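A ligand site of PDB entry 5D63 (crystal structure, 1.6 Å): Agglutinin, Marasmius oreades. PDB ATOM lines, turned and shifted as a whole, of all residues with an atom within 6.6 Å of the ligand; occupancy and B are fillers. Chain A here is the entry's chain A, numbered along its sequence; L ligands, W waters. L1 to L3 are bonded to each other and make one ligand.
The side-chain carboxylate of Asp 20 sits at hydrogen-bond distance from an oxygen (O6) of LG2 L2. OD1 of Asn 43 is in hydrogen-bond range of O1 of LG3 L3, 2.7 Å away. N of Thr 38 is in hydrogen-bond range of O2 of LG3 L3 (3.2 Å). OG1 of Thr 38 lies within hydrogen-bond range of O2 of LG3 L3 (2.7 Å). The backbone NH (N) of Asp 23 sits at hydrogen-bond distance from an oxygen (O6) of LG2 L2, 2.8 Å away. A ring nitrogen (ND1) of His 45 lies within hydrogen-bond range of an oxygen (O6) of LG2 L2 (3.0 Å). The indole nitrogen (NE1) of Trp 35 lies within hydrogen-bond range of an oxygen (O4) of LG3 L3. The backbone carbonyl oxygen (O) of Gln 36 lies within hydrogen-bond range of an oxygen (O3) of LG3 L3 (3.2 Å).
The side-chain amide nitrogen (NE2) of Gln 46 is in hydrogen-bond range of the side-chain carboxylate (OD2) of Asp 20 (2.9 Å). The backbone NH of Val 33 is in hydrogen-bond range of the backbone carbonyl oxygen of Asp 20 (2.8 Å). ND2 of Asn 43 sits at hydrogen-bond distance from OG1 of Thr 41 (3.3 Å). The backbone carbonyl oxygen of Thr 38 is in hydrogen-bond range of the side-chain hydroxyl of Thr 41. The backbone carbonyl oxygen (O) of His 45 is in hydrogen-bond range of the backbone NH (N) of Leu 21, 3.1 Å away. A ring nitrogen (ND1) of His 45 sits at hydrogen-bond distance from the backbone NH (N) of Gly 24, 3.4 Å away. NE2 of Gln 46 lies within hydrogen-bond range of O of Gln 36. The side-chain amide nitrogen (NE2) of Gln 36 sits at hydrogen-bond distance from the side-chain carboxylate (OD2) of Asp 131, 2.8 Å away.
Residues that only touch the ligand: Leu 21 (3.5 Å), Lys 22 (3.6 Å), Phe 37 (3.5 Å), Trp 44 (3.99 Å) and Gln 46 (3.8 Å). Hydrophobic or aromatic side chains that line the ligand: Trp 35, Trp 44 and His 45. Of the 20 residues printed, 12 come within 4 Å of the ligand.
Water W4 lies within hydrogen-bond range of an oxygen (O2) of LG3 L3, the side-chain hydroxyl of Thr 41, the backbone carbonyl oxygen of Ile 42 and the side-chain amide oxygen of Asn 43. Water W6 lies within hydrogen-bond range of O4 of LG2 L2 (2.8 Å), N of His 45 (2.8 Å) and N of Trp 44 (3.3 Å). Water W2 bridges the side-chain carboxylate (OD2) of Asp 131 and an oxygen (O5) of LG3 L3. Water W5 lies within hydrogen-bond range of an oxygen (O1) of LG3 L3 (3.0 Å), the backbone NH of Trp 44 (3.1 Å) and the backbone carbonyl oxygen of Ile 42 (3.2 Å).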
ATOM      1  N   HIS A   9     -28.539 -16.008 -29.771  1.00  0.00           N
ATOM      2  CA  HIS A   9     -28.178 -16.551 -28.452  1.00  0.00           C
ATOM      3  C   HIS A   9     -27.242 -17.703 -28.757  1.00  0.00           C
ATOM      4  O   HIS A   9     -27.604 -18.591 -29.547  1.00  0.00           O
ATOM      5  CB  HIS A   9     -29.440 -17.033 -27.769  1.00  0.00           C
ATOM      6  CG  HIS A   9     -29.218 -17.492 -26.362  1.00  0.00           C
ATOM      7  ND1 HIS A   9     -29.221 -18.841 -25.983  1.00  0.00           N
ATOM      8  CD2 HIS A   9     -28.890 -16.790 -25.246  1.00  0.00           C
ATOM      9  CE1 HIS A   9     -28.905 -18.926 -24.721  1.00  0.00           C
ATOM     10  NE2 HIS A   9     -28.733 -17.699 -24.236  1.00  0.00           N
ATOM     11  N   ASP A  20     -21.785 -15.071 -22.615  1.00  0.00           N
ATOM     12  CA  ASP A  20     -22.378 -14.075 -21.762  1.00  0.00           C
ATOM     13  C   ASP A  20     -21.321 -12.957 -21.503  1.00  0.00           C
ATOM     14  O   ASP A  20     -20.179 -13.156 -21.142  1.00  0.00           O
ATOM     15  CB  ASP A  20     -22.824 -14.831 -20.506  1.00  0.00           C
ATOM     16  CG  ASP A  20     -23.476 -13.936 -19.408  1.00  0.00           C
ATOM     17  OD1 ASP A  20     -22.856 -12.942 -18.916  1.00  0.00           O
ATOM     18  OD2 ASP A  20     -24.632 -14.229 -18.995  1.00  0.00           O
ATOM     19  N   LEU A  21     -21.731 -11.732 -21.708  1.00  0.00           N
ATOM     20  CA  LEU A  21     -20.901 -10.577 -21.367  1.00  0.00           C
ATOM     21  C   LEU A  21     -21.146 -10.259 -19.925  1.00  0.00           C
ATOM     22  O   LEU A  21     -22.291  -9.894 -19.496  1.00  0.00           O
ATOM     23  CB  LEU A  21     -21.296  -9.377 -22.221  1.00  0.00           C
ATOM     24  CG  LEU A  21     -20.518  -8.117 -21.936  1.00  0.00           C
ATOM     25  CD1 LEU A  21     -18.995  -8.230 -22.200  1.00  0.00           C
ATOM     26  CD2 LEU A  21     -21.036  -6.925 -22.766  1.00  0.00           C
ATOM     27  N   LYS A  22     -20.117 -10.442 -19.101  1.00  0.00           N
ATOM     28  CA  LYS A  22     -20.331 -10.547 -17.640  1.00  0.00           C
ATOM     29  C   LYS A  22     -20.958  -9.252 -17.081  1.00  0.00           C
ATOM     30  O   LYS A  22     -20.439  -8.132 -17.257  1.00  0.00           O
ATOM     31  CB  LYS A  22     -19.018 -10.891 -16.944  1.00  0.00           C
ATOM     32  CG  LYS A  22     -19.246 -11.567 -15.586  1.00  0.00           C
ATOM     33  CD  LYS A  22     -17.956 -11.921 -14.838  1.00  0.00           C
ATOM     34  CE  LYS A  22     -18.358 -12.555 -13.477  1.00  0.00           C
ATOM     35  NZ  LYS A  22     -17.069 -13.251 -12.906  1.00  0.00           N
ATOM     36  N   ASP A  23     -22.049  -9.399 -16.329  1.00  0.00           N
ATOM     37  CA  ASP A  23     -22.841  -8.299 -15.793  1.00  0.00           C
ATOM     38  C   ASP A  23     -23.337  -7.288 -16.805  1.00  0.00           C
ATOM     39  O   ASP A  23     -23.791  -6.234 -16.452  1.00  0.00           O
ATOM     40  CB  ASP A  23     -22.066  -7.614 -14.683  1.00  0.00           C
ATOM     41  CG  ASP A  23     -22.992  -6.988 -13.624  1.00  0.00           C
ATOM     42  OD1 ASP A  23     -24.081  -7.535 -13.332  1.00  0.00           O
ATOM     43  OD2 ASP A  23     -22.653  -5.847 -13.193  1.00  0.00           O
ATOM     44  N   GLY A  24     -23.359  -7.657 -18.067  1.00  0.00           N
ATOM     45  CA  GLY A  24     -23.779  -6.760 -19.155  1.00  0.00           C
ATOM     46  C   GLY A  24     -22.917  -5.523 -19.206  1.00  0.00           C
ATOM     47  O   GLY A  24     -23.338  -4.548 -19.833  1.00  0.00           O
ATOM     48  N   VAL A  33     -17.918 -14.787 -20.857  1.00  0.00           N
ATOM     49  CA  VAL A  33     -17.812 -16.018 -20.111  1.00  0.00           C
ATOM     50  C   VAL A  33     -18.926 -16.979 -20.482  1.00  0.00           C
ATOM     51  O   VAL A  33     -19.978 -16.580 -21.016  1.00  0.00           O
ATOM     52  CB  VAL A  33     -17.937 -15.804 -18.566  1.00  0.00           C
ATOM     53  CG1 VAL A  33     -16.692 -15.027 -18.127  1.00  0.00           C
ATOM     54  CG2 VAL A  33     -19.187 -15.037 -18.238  1.00  0.00           C
ATOM     55  N   TRP A  35     -22.200 -19.126 -19.279  1.00  0.00           N
ATOM     56  CA  TRP A  35     -23.170 -18.910 -18.185  1.00  0.00           C
ATOM     57  C   TRP A  35     -24.453 -19.707 -18.566  1.00  0.00           C
ATOM     58  O   TRP A  35     -24.883 -19.662 -19.713  1.00  0.00           O
ATOM     59  CB  TRP A  35     -23.487 -17.425 -18.057  1.00  0.00           C
ATOM     60  CG  TRP A  35     -23.946 -17.037 -16.662  1.00  0.00           C
ATOM     61  CD1 TRP A  35     -25.193 -17.243 -16.098  1.00  0.00           C
ATOM     62  CD2 TRP A  35     -23.147 -16.428 -15.635  1.00  0.00           C
ATOM     63  NE1 TRP A  35     -25.221 -16.807 -14.797  1.00  0.00           N
ATOM     64  CE2 TRP A  35     -23.972 -16.313 -14.466  1.00  0.00           C
ATOM     65  CE3 TRP A  35     -21.817 -16.024 -15.568  1.00  0.00           C
ATOM     66  CZ2 TRP A  35     -23.514 -15.771 -13.279  1.00  0.00           C
ATOM     67  CZ3 TRP A  35     -21.359 -15.504 -14.353  1.00  0.00           C
ATOM     68  CH2 TRP A  35     -22.196 -15.412 -13.218  1.00  0.00           C
ATOM     69  N   GLN A  36     -25.134 -20.235 -17.586  1.00  0.00           N
ATOM     70  CA  GLN A  36     -26.390 -20.882 -17.832  1.00  0.00           C
ATOM     71  C   GLN A  36     -27.467 -19.925 -18.260  1.00  0.00           C
ATOM     72  O   GLN A  36     -27.381 -18.754 -18.027  1.00  0.00           O
ATOM     73  CB  GLN A  36     -26.870 -21.664 -16.603  1.00  0.00           C
ATOM     74  CG  GLN A  36     -27.273 -20.835 -15.403  1.00  0.00           C
ATOM     75  CD  GLN A  36     -27.683 -21.746 -14.254  1.00  0.00           C
ATOM     76  OE1 GLN A  36     -28.659 -22.470 -14.340  1.00  0.00           O
ATOM     77  NE2 GLN A  36     -26.884 -21.777 -13.250  1.00  0.00           N
ATOM     78  N   PHE A  37     -28.558 -20.453 -18.795  1.00  0.00           N
ATOM     79  CA  PHE A  37     -29.598 -19.618 -19.372  1.00  0.00           C
ATOM     80  C   PHE A  37     -30.971 -20.243 -19.187  1.00  0.00           C
ATOM     81  O   PHE A  37     -31.061 -21.395 -18.785  1.00  0.00           O
ATOM     82  CB  PHE A  37     -29.395 -19.421 -20.928  1.00  0.00           C
ATOM     83  CG  PHE A  37     -29.480 -20.682 -21.758  1.00  0.00           C
ATOM     84  CD1 PHE A  37     -28.370 -21.459 -21.961  1.00  0.00           C
ATOM     85  CD2 PHE A  37     -30.652 -21.031 -22.371  1.00  0.00           C
ATOM     86  CE1 PHE A  37     -28.426 -22.622 -22.728  1.00  0.00           C
ATOM     87  CE2 PHE A  37     -30.752 -22.213 -23.153  1.00  0.00           C
ATOM     88  CZ  PHE A  37     -29.618 -22.967 -23.294  1.00  0.00           C
ATOM     89  N   THR A  38     -31.967 -19.408 -19.424  1.00  0.00           N
ATOM     90  CA  THR A  38     -33.399 -19.882 -19.275  1.00  0.00           C
ATOM     91  C   THR A  38     -34.057 -19.754 -20.630  1.00  0.00           C
ATOM     92  O   THR A  38     -34.158 -18.672 -21.199  1.00  0.00           O
ATOM     93  CB  THR A  38     -34.169 -19.020 -18.212  1.00  0.00           C
ATOM     94  OG1 THR A  38     -33.411 -19.019 -16.960  1.00  0.00           O
ATOM     95  CG2 THR A  38     -35.528 -19.609 -17.998  1.00  0.00           C
ATOM     96  N   PRO A  39     -34.512 -20.864 -21.199  1.00  0.00           N
ATOM     97  CA  PRO A  39     -35.177 -20.787 -22.528  1.00  0.00           C
ATOM     98  C   PRO A  39     -36.453 -19.989 -22.478  1.00  0.00           C
ATOM     99  O   PRO A  39     -37.088 -19.881 -21.433  1.00  0.00           O
ATOM    100  CB  PRO A  39     -35.524 -22.224 -22.878  1.00  0.00           C
ATOM    101  CG  PRO A  39     -35.093 -23.024 -21.713  1.00  0.00           C
ATOM    102  CD  PRO A  39     -34.453 -22.217 -20.654  1.00  0.00           C
ATOM    103  N   THR A  41     -37.017 -16.831 -22.492  1.00  0.00           N
ATOM    104  CA  THR A  41     -36.872 -15.586 -21.749  1.00  0.00           C
ATOM    105  C   THR A  41     -35.996 -14.673 -22.562  1.00  0.00           C
ATOM    106  O   THR A  41     -35.321 -15.152 -23.467  1.00  0.00           O
ATOM    107  CB  THR A  41     -36.218 -15.701 -20.354  1.00  0.00           C
ATOM    108  OG1 THR A  41     -34.808 -16.036 -20.529  1.00  0.00           O
ATOM    109  CG2 THR A  41     -36.915 -16.682 -19.484  1.00  0.00           C
ATOM    110  N   ILE A  42     -36.001 -13.388 -22.260  1.00  0.00           N
ATOM    111  CA  ILE A  42     -34.895 -12.538 -22.658  1.00  0.00           C
ATOM    112  C   ILE A  42     -33.722 -12.832 -21.714  1.00  0.00           C
ATOM    113  O   ILE A  42     -33.792 -12.551 -20.500  1.00  0.00           O
ATOM    114  CB  ILE A  42     -35.248 -11.037 -22.620  1.00  0.00           C
ATOM    115  CG1 ILE A  42     -36.411 -10.693 -23.611  1.00  0.00           C
ATOM    116  CG2 ILE A  42     -33.973 -10.174 -22.778  1.00  0.00           C
ATOM    117  CD1 ILE A  42     -36.178 -11.077 -25.033  1.00  0.00           C
ATOM    118  N   ASN A  43     -32.620 -13.346 -22.284  1.00  0.00           N
ATOM    119  CA  ASN A  43     -31.322 -13.540 -21.550  1.00  0.00           C
ATOM    120  C   ASN A  43     -30.483 -12.308 -21.754  1.00  0.00           C
ATOM    121  O   ASN A  43     -29.783 -12.158 -22.799  1.00  0.00           O
ATOM    122  CB  ASN A  43     -30.628 -14.833 -22.041  1.00  0.00           C
ATOM    123  CG  ASN A  43     -31.359 -16.078 -21.574  1.00  0.00           C
ATOM    124  OD1 ASN A  43     -31.284 -16.463 -20.403  1.00  0.00           O
ATOM    125  ND2 ASN A  43     -32.145 -16.675 -22.437  1.00  0.00           N
ATOM    126  N   TRP A  44     -30.670 -11.339 -20.840  1.00  0.00           N
ATOM    127  CA  TRP A  44     -30.247  -9.969 -20.994  1.00  0.00           C
ATOM    128  C   TRP A  44     -28.784  -9.759 -21.369  1.00  0.00           C
ATOM    129  O   TRP A  44     -28.465  -8.801 -22.133  1.00  0.00           O
ATOM    130  CB  TRP A  44     -30.589  -9.166 -19.718  1.00  0.00           C
ATOM    131  CG  TRP A  44     -32.025  -8.842 -19.618  1.00  0.00           C
ATOM    132  CD1 TRP A  44     -33.013  -9.529 -18.942  1.00  0.00           C
ATOM    133  CD2 TRP A  44     -32.685  -7.766 -20.305  1.00  0.00           C
ATOM    134  NE1 TRP A  44     -34.209  -8.892 -19.117  1.00  0.00           N
ATOM    135  CE2 TRP A  44     -34.050  -7.844 -19.979  1.00  0.00           C
ATOM    136  CE3 TRP A  44     -32.230  -6.759 -21.118  1.00  0.00           C
ATOM    137  CZ2 TRP A  44     -34.976  -6.925 -20.459  1.00  0.00           C
ATOM    138  CZ3 TRP A  44     -33.140  -5.854 -21.609  1.00  0.00           C
ATOM    139  CH2 TRP A  44     -34.514  -5.977 -21.311  1.00  0.00           C
ATOM    140  N   HIS A  45     -27.860 -10.595 -20.889  1.00  0.00           N
ATOM    141  CA  HIS A  45     -26.455 -10.394 -21.205  1.00  0.00           C
ATOM    142  C   HIS A  45     -25.898 -11.277 -22.271  1.00  0.00           C
ATOM    143  O   HIS A  45     -24.678 -11.325 -22.535  1.00  0.00           O
ATOM    144  CB  HIS A  45     -25.614 -10.525 -19.897  1.00  0.00           C
ATOM    145  CG  HIS A  45     -26.108  -9.633 -18.787  1.00  0.00           C
ATOM    146  ND1 HIS A  45     -25.875  -9.909 -17.441  1.00  0.00           N
ATOM    147  CD2 HIS A  45     -26.752  -8.464 -18.830  1.00  0.00           C
ATOM    148  CE1 HIS A  45     -26.358  -8.913 -16.713  1.00  0.00           C
ATOM    149  NE2 HIS A  45     -26.920  -8.034 -17.512  1.00  0.00           N
ATOM    150  N   GLN A  46     -26.745 -12.054 -22.952  1.00  0.00           N
ATOM    151  CA  GLN A  46     -26.369 -13.170 -23.813  1.00  0.00           C
ATOM    152  C   GLN A  46     -26.911 -13.056 -25.237  1.00  0.00           C
ATOM    153  O   GLN A  46     -27.035 -14.053 -25.923  1.00  0.00           O
ATOM    154  CB  GLN A  46     -26.925 -14.467 -23.217  1.00  0.00           C
ATOM    155  CG  GLN A  46     -26.446 -14.693 -21.779  1.00  0.00           C
ATOM    156  CD  GLN A  46     -26.964 -15.988 -21.151  1.00  0.00           C
ATOM    157  OE1 GLN A  46     -27.859 -16.675 -21.695  1.00  0.00           O
ATOM    158  NE2 GLN A  46     -26.450 -16.307 -19.942  1.00  0.00           N
ATOM    159  N   PHE A  66     -27.272  -5.677 -25.235  1.00  0.00           N
ATOM    160  CA  PHE A  66     -27.424  -4.883 -23.997  1.00  0.00           C
ATOM    161  C   PHE A  66     -26.343  -3.831 -23.833  1.00  0.00           C
ATOM    162  O   PHE A  66     -26.679  -2.661 -23.595  1.00  0.00           O
ATOM    163  CB  PHE A  66     -27.431  -5.799 -22.792  1.00  0.00           C
ATOM    164  CG  PHE A  66     -27.681  -5.089 -21.495  1.00  0.00           C
ATOM    165  CD1 PHE A  66     -28.971  -4.601 -21.168  1.00  0.00           C
ATOM    166  CD2 PHE A  66     -26.629  -4.798 -20.632  1.00  0.00           C
ATOM    167  CE1 PHE A  66     -29.181  -3.890 -20.009  1.00  0.00           C
ATOM    168  CE2 PHE A  66     -26.858  -4.177 -19.412  1.00  0.00           C
ATOM    169  CZ  PHE A  66     -28.144  -3.769 -19.075  1.00  0.00           C
ATOM    170  N   ASP A 131     -20.980 -21.312 -14.113  1.00  0.00           N
ATOM    171  CA  ASP A 131     -21.284 -19.931 -14.430  1.00  0.00           C
ATOM    172  C   ASP A 131     -20.029 -19.083 -14.215  1.00  0.00           C
ATOM    173  O   ASP A 131     -19.421 -19.049 -13.093  1.00  0.00           O
ATOM    174  CB  ASP A 131     -22.415 -19.423 -13.584  1.00  0.00           C
ATOM    175  CG  ASP A 131     -23.734 -20.139 -13.870  1.00  0.00           C
ATOM    176  OD1 ASP A 131     -23.892 -20.609 -14.985  1.00  0.00           O
ATOM    177  OD2 ASP A 131     -24.665 -20.094 -12.965  1.00  0.00           O
HETATM  178  C1  LIG L   1     -30.323 -12.354 -14.698  1.00  0.00           C
HETATM  179  C2  LIG L   1     -31.299 -12.435 -13.524  1.00  0.00           C
HETATM  180  C3  LIG L   1     -31.248 -11.103 -12.726  1.00  0.00           C
HETATM  181  C4  LIG L   1     -31.477  -9.936 -13.678  1.00  0.00           C
HETATM  182  C5  LIG L   1     -30.375  -9.956 -14.763  1.00  0.00           C
HETATM  183  C6  LIG L   1     -30.543  -8.810 -15.747  1.00  0.00           C
HETATM  184  O1  LIG L   1     -30.894 -13.536 -12.709  1.00  0.00           O
HETATM  185  O2  LIG L   1     -32.366 -11.217 -11.815  1.00  0.00           O
HETATM  186  O3  LIG L   1     -32.799  -9.878 -14.286  1.00  0.00           O
HETATM  187  O4  LIG L   1     -30.454 -11.182 -15.528  1.00  0.00           O
HETATM  188  C1  LG2 L   2     -26.803 -11.610 -14.080  1.00  0.00           C
HETATM  189  C2  LG2 L   2     -27.879 -12.212 -15.014  1.00  0.00           C
HETATM  190  C3  LG2 L   2     -27.457 -13.620 -15.458  1.00  0.00           C
HETATM  191  C4  LG2 L   2     -26.105 -13.665 -16.110  1.00  0.00           C
HETATM  192  C5  LG2 L   2     -25.085 -12.863 -15.224  1.00  0.00           C
HETATM  193  C6  LG2 L   2     -23.658 -12.741 -15.781  1.00  0.00           C
HETATM  194  O1  LG2 L   2     -27.101 -10.222 -13.963  1.00  0.00           O
HETATM  195  O2  LG2 L   2     -29.021 -12.355 -14.111  1.00  0.00           O
HETATM  196  O3  LG2 L   2     -28.479 -14.181 -16.322  1.00  0.00           O
HETATM  197  O4  LG2 L   2     -26.168 -12.980 -17.374  1.00  0.00           O
HETATM  198  O5  LG2 L   2     -25.598 -11.536 -14.875  1.00  0.00           O
HETATM  199  O6  LG2 L   2     -23.597 -11.738 -16.819  1.00  0.00           O
HETATM  200  C1  LG3 L   3     -28.283 -15.532 -16.742  1.00  0.00           C
HETATM  201  C2  LG3 L   3     -29.531 -15.926 -17.569  1.00  0.00           C
HETATM  202  C3  LG3 L   3     -30.735 -16.268 -16.693  1.00  0.00           C
HETATM  203  C4  LG3 L   3     -30.353 -17.207 -15.521  1.00  0.00           C
HETATM  204  C5  LG3 L   3     -29.211 -16.550 -14.735  1.00  0.00           C
HETATM  205  C6  LG3 L   3     -28.658 -17.308 -13.602  1.00  0.00           C
HETATM  206  O1  LG3 L   3     -29.940 -15.000 -18.560  1.00  0.00           O
HETATM  207  O2  LG3 L   3     -31.850 -16.822 -17.470  1.00  0.00           O
HETATM  208  O3  LG3 L   3     -29.897 -18.458 -16.068  1.00  0.00           O
HETATM  209  O4  LG3 L   3     -28.058 -16.403 -15.664  1.00  0.00           O
HETATM  210  O5  LG3 L   3     -27.565 -16.599 -12.945  1.00  0.00           O
HETATM  211  O   HOH W   1     -32.256 -15.829 -13.251  1.00  0.00           O
HETATM  212  O   HOH W   2     -25.552 -17.903 -11.241  1.00  0.00           O
HETATM  213  O   HOH W   3     -33.078  -8.526 -11.005  1.00  0.00           O
HETATM  214  O   HOH W   4     -33.323 -14.904 -18.454  1.00  0.00           O
HETATM  215  O   HOH W   5     -31.610 -12.582 -18.163  1.00  0.00           O
HETATM  216  O   HOH W   6     -28.207 -12.848 -19.232  1.00  0.00           O
HETATM  217  O   HOH W   7     -33.602 -11.868 -16.217  1.00  0.00           O
HETATM  218  O   HOH W   8     -28.362 -14.268 -11.655  1.00  0.00           O
